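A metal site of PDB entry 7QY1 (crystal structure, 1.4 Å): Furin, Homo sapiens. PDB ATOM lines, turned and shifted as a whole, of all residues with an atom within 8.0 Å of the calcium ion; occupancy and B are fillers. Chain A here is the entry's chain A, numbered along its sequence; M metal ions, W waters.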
ATOM      1  N   LYS A  51     -13.285   5.294  10.049  1.00  0.00           N
ATOM      2  CA  LYS A  51     -12.292   5.419   8.992  1.00  0.00           C
ATOM      3  C   LYS A  51     -12.540   6.632   8.123  1.00  0.00           C
ATOM      4  O   LYS A  51     -11.602   7.131   7.480  1.00  0.00           O
ATOM      5  CB  LYS A  51     -12.235   4.139   8.164  1.00  0.00           C
ATOM      6  CG  LYS A  51     -13.450   3.804   7.352  1.00  0.00           C
ATOM      7  CD  LYS A  51     -13.356   2.363   6.831  1.00  0.00           C
ATOM      8  CE  LYS A  51     -14.628   1.960   6.132  1.00  0.00           C
ATOM      9  NZ  LYS A  51     -15.745   1.850   7.092  1.00  0.00           N
ATOM     10  N   PHE A  66      -9.347  -4.683  10.755  1.00  0.00           N
ATOM     11  CA  PHE A  66     -10.228  -5.839  10.673  1.00  0.00           C
ATOM     12  C   PHE A  66     -11.296  -5.734  11.760  1.00  0.00           C
ATOM     13  O   PHE A  66     -11.151  -4.974  12.719  1.00  0.00           O
ATOM     14  CB  PHE A  66      -9.443  -7.149  10.826  1.00  0.00           C
ATOM     15  CG  PHE A  66     -10.088  -8.294  10.122  1.00  0.00           C
ATOM     16  CD1 PHE A  66      -9.944  -8.451   8.764  1.00  0.00           C
ATOM     17  CD2 PHE A  66     -10.854  -9.198  10.822  1.00  0.00           C
ATOM     18  CE1 PHE A  66     -10.560  -9.518   8.109  1.00  0.00           C
ATOM     19  CE2 PHE A  66     -11.454 -10.246  10.178  1.00  0.00           C
ATOM     20  CZ  PHE A  66     -11.310 -10.402   8.821  1.00  0.00           C
ATOM     21  N   ASP A  67     -12.373  -6.485  11.567  1.00  0.00           N
ATOM     22  CA  ASP A  67     -13.465  -6.565  12.544  1.00  0.00           C
ATOM     23  C   ASP A  67     -13.558  -8.019  12.988  1.00  0.00           C
ATOM     24  O   ASP A  67     -14.158  -8.849  12.308  1.00  0.00           O
ATOM     25  CB  ASP A  67     -14.761  -6.070  11.930  1.00  0.00           C
ATOM     26  CG  ASP A  67     -15.928  -6.082  12.892  1.00  0.00           C
ATOM     27  OD1 ASP A  67     -15.846  -6.681  13.992  1.00  0.00           O
ATOM     28  OD2 ASP A  67     -16.959  -5.487  12.499  1.00  0.00           O
ATOM     29  N   VAL A  68     -12.957  -8.334  14.147  1.00  0.00           N
ATOM     30  CA  VAL A  68     -13.025  -9.700  14.680  1.00  0.00           C
ATOM     31  C   VAL A  68     -14.263  -9.945  15.524  1.00  0.00           C
ATOM     32  O   VAL A  68     -14.505 -11.090  15.944  1.00  0.00           O
ATOM     33  CB  VAL A  68     -11.763 -10.082  15.475  1.00  0.00           C
ATOM     34  CG1 VAL A  68     -10.535 -10.031  14.569  1.00  0.00           C
ATOM     35  CG2 VAL A  68     -11.599  -9.211  16.702  1.00  0.00           C
ATOM     36  N   ASN A  69     -15.048  -8.906  15.823  1.00  0.00           N
ATOM     37  CA  ASN A  69     -16.311  -9.114  16.529  1.00  0.00           C
ATOM     38  C   ASN A  69     -17.395  -9.616  15.563  1.00  0.00           C
ATOM     39  O   ASN A  69     -18.150 -10.540  15.895  1.00  0.00           O
ATOM     40  CB  ASN A  69     -16.785  -7.831  17.221  1.00  0.00           C
ATOM     41  CG  ASN A  69     -15.881  -7.396  18.387  1.00  0.00           C
ATOM     42  OD1 ASN A  69     -15.542  -6.212  18.519  1.00  0.00           O
ATOM     43  ND2 ASN A  69     -15.495  -8.352  19.235  1.00  0.00           N
ATOM     44  N   ASP A  70     -17.469  -9.048  14.366  1.00  0.00           N
ATOM     45  CA  ASP A  70     -18.449  -9.459  13.372  1.00  0.00           C
ATOM     46  C   ASP A  70     -17.838 -10.240  12.220  1.00  0.00           C
ATOM     47  O   ASP A  70     -18.550 -10.621  11.301  1.00  0.00           O
ATOM     48  CB  ASP A  70     -19.202  -8.244  12.796  1.00  0.00           C
ATOM     49  CG  ASP A  70     -20.312  -7.729  13.701  1.00  0.00           C
ATOM     50  OD1 ASP A  70     -20.806  -8.493  14.558  1.00  0.00           O
ATOM     51  OD2 ASP A  70     -20.702  -6.556  13.550  1.00  0.00           O
ATOM     52  N   GLN A  71     -16.520 -10.475  12.231  1.00  0.00           N
ATOM     53  CA  GLN A  71     -15.864 -11.305  11.210  1.00  0.00           C
ATOM     54  C   GLN A  71     -16.008 -10.702   9.802  1.00  0.00           C
ATOM     55  O   GLN A  71     -16.545 -11.307   8.876  1.00  0.00           O
ATOM     56  CB  GLN A  71     -16.348 -12.754  11.282  1.00  0.00           C
ATOM     57  CG  GLN A  71     -16.198 -13.355  12.678  1.00  0.00           C
ATOM     58  CD  GLN A  71     -16.143 -14.866  12.693  1.00  0.00           C
ATOM     59  N   ASP A  72     -15.474  -9.497   9.653  1.00  0.00           N
ATOM     60  CA  ASP A  72     -15.451  -8.815   8.361  1.00  0.00           C
ATOM     61  C   ASP A  72     -14.289  -7.847   8.344  1.00  0.00           C
ATOM     62  O   ASP A  72     -13.647  -7.617   9.384  1.00  0.00           O
ATOM     63  CB  ASP A  72     -16.799  -8.133   8.051  1.00  0.00           C
ATOM     64  CG  ASP A  72     -17.121  -6.951   8.990  1.00  0.00           C
ATOM     65  OD1 ASP A  72     -16.398  -5.956   8.949  1.00  0.00           O
ATOM     66  OD2 ASP A  72     -18.123  -7.009   9.727  1.00  0.00           O
ATOM     67  N   PRO A  73     -13.957  -7.276   7.181  1.00  0.00           N
ATOM     68  CA  PRO A  73     -12.749  -6.435   7.132  1.00  0.00           C
ATOM     69  C   PRO A  73     -12.931  -5.027   7.641  1.00  0.00           C
ATOM     70  O   PRO A  73     -11.930  -4.314   7.780  1.00  0.00           O
ATOM     71  CB  PRO A  73     -12.383  -6.387   5.637  1.00  0.00           C
ATOM     72  CG  PRO A  73     -13.280  -7.312   4.970  1.00  0.00           C
ATOM     73  CD  PRO A  73     -14.480  -7.541   5.837  1.00  0.00           C
ATOM     74  N   ASP A  74     -14.173  -4.601   7.922  1.00  0.00           N
ATOM     75  CA  ASP A  74     -14.504  -3.195   8.100  1.00  0.00           C
ATOM     76  C   ASP A  74     -14.675  -2.899   9.582  1.00  0.00           C
ATOM     77  O   ASP A  74     -15.657  -3.374  10.172  1.00  0.00           O
ATOM     78  CB  ASP A  74     -15.806  -2.902   7.360  1.00  0.00           C
ATOM     79  CG  ASP A  74     -16.224  -1.465   7.430  1.00  0.00           C
ATOM     80  OD1 ASP A  74     -15.639  -0.693   8.217  1.00  0.00           O
ATOM     81  OD2 ASP A  74     -17.152  -1.087   6.678  1.00  0.00           O
ATOM     82  N   PRO A  75     -13.761  -2.103  10.209  1.00  0.00           N
ATOM     83  CA  PRO A  75     -13.819  -1.894  11.669  1.00  0.00           C
ATOM     84  C   PRO A  75     -14.652  -0.694  12.083  1.00  0.00           C
ATOM     85  O   PRO A  75     -14.459  -0.151  13.186  1.00  0.00           O
ATOM     86  CB  PRO A  75     -12.352  -1.621  12.003  1.00  0.00           C
ATOM     87  CG  PRO A  75     -11.917  -0.780  10.792  1.00  0.00           C
ATOM     88  CD  PRO A  75     -12.571  -1.472   9.607  1.00  0.00           C
ATOM     89  N   GLN A  76     -15.550  -0.247  11.217  1.00  0.00           N
ATOM     90  CA  GLN A  76     -16.360   0.917  11.558  1.00  0.00           C
ATOM     91  C   GLN A  76     -17.096   0.668  12.876  1.00  0.00           C
ATOM     92  O   GLN A  76     -17.619  -0.434  13.108  1.00  0.00           O
ATOM     93  CB  GLN A  76     -17.360   1.192  10.438  1.00  0.00           C
ATOM     94  CG  GLN A  76     -18.025   2.553  10.519  1.00  0.00           C
ATOM     95  CD  GLN A  76     -17.126   3.691  10.041  1.00  0.00           C
ATOM     96  OE1 GLN A  76     -16.075   3.470   9.433  1.00  0.00           O
ATOM     97  NE2 GLN A  76     -17.536   4.919  10.332  1.00  0.00           N
ATOM     98  N   PRO A  77     -17.143   1.661  13.762  1.00  0.00           N
ATOM     99  CA  PRO A  77     -17.791   1.445  15.058  1.00  0.00           C
ATOM    100  C   PRO A  77     -19.297   1.296  14.945  1.00  0.00           C
ATOM    101  O   PRO A  77     -19.935   1.760  13.995  1.00  0.00           O
ATOM    102  CB  PRO A  77     -17.446   2.715  15.859  1.00  0.00           C
ATOM    103  CG  PRO A  77     -16.261   3.328  15.154  1.00  0.00           C
ATOM    104  CD  PRO A  77     -16.456   2.958  13.691  1.00  0.00           C
ATOM    105  N   ARG A  78     -19.866   0.673  15.973  1.00  0.00           N
ATOM    106  CA  ARG A  78     -21.310   0.602  16.162  1.00  0.00           C
ATOM    107  C   ARG A  78     -21.750   1.859  16.885  1.00  0.00           C
ATOM    108  O   ARG A  78     -21.337   2.096  18.029  1.00  0.00           O
ATOM    109  CB  ARG A  78     -21.641  -0.640  16.990  1.00  0.00           C
ATOM    110  CG  ARG A  78     -23.110  -0.834  17.328  1.00  0.00           C
ATOM    111  CD  ARG A  78     -23.349  -2.180  17.998  1.00  0.00           C
ATOM    112  NE  ARG A  78     -22.597  -2.240  19.246  1.00  0.00           N
ATOM    113  CZ  ARG A  78     -23.076  -1.899  20.430  1.00  0.00           C
ATOM    114  NH1 ARG A  78     -24.330  -1.466  20.576  1.00  0.00           N
ATOM    115  NH2 ARG A  78     -22.268  -1.941  21.476  1.00  0.00           N
ATOM    116  N   ARG A 118     -11.542  -3.881  15.348  1.00  0.00           N
ATOM    117  CA  ARG A 118     -12.755  -3.848  16.136  1.00  0.00           C
ATOM    118  C   ARG A 118     -12.809  -5.195  16.826  1.00  0.00           C
ATOM    119  O   ARG A 118     -13.135  -6.210  16.213  1.00  0.00           O
ATOM    120  CB  ARG A 118     -13.975  -3.607  15.249  1.00  0.00           C
ATOM    121  CG  ARG A 118     -15.284  -3.520  16.008  1.00  0.00           C
ATOM    122  CD  ARG A 118     -16.477  -3.080  15.079  1.00  0.00           C
ATOM    123  NE  ARG A 118     -17.710  -3.114  15.857  1.00  0.00           N
ATOM    124  CZ  ARG A 118     -18.653  -4.041  15.771  1.00  0.00           C
ATOM    125  NH1 ARG A 118     -18.584  -5.021  14.866  1.00  0.00           N
ATOM    126  NH2 ARG A 118     -19.706  -3.973  16.585  1.00  0.00           N
HETATM  127 CA    CA M   1     -17.726  -4.615  10.488  1.00  0.00          CA
HETATM  128  O   HOH W   1     -18.872  -3.823   8.579  1.00  0.00           O
HETATM  129  O   HOH W   2     -18.310  -2.474  11.335  1.00  0.00           O
HETATM  130  O   HOH W   3     -19.962  -5.064  11.406  1.00  0.00           O
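The side-chain carboxylate (OD1) of Asp 67 is in salt-bridge range of the guanidinium group (NH1) of Arg 118 (3.3 Å).
The side-chain amino group (NZ) of Lys 51 is in salt-bridge range of the side-chain carboxylate (OD1) of Asp 74, 2.8 Å away.
N of Asn 69 sits at hydrogen-bond distance from OD1 of Asp 67 (3.0 Å).
The side-chain carboxylate (OD1) of Asp 67 sits at hydrogen-bond distance from the backbone NH (N) of Asp 70 (2.9 Å).
The side-chain carboxylate of Asp 74 sits at hydrogen-bond distance from the backbone NH of Gln 76 (3.0 Å).
Of the 15 residues printed, 3 come within 4 Å of the calcium ion.
Along chain A the residues within 4 Å of the calcium ion span positions 67 to 74.
The calcium ion is bound by OD2 of Asp 67 (2.3 Å), water W1 (2.4 Å), water W2 (2.4 Å), O of Asp 74 (2.4 Å), OD1 of Asp 72 (2.4 Å), water W3 (2.5 Å) and OD2 of Asp 72 (2.5 Å).
The calcium ion has seven donor atoms within binding distance.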
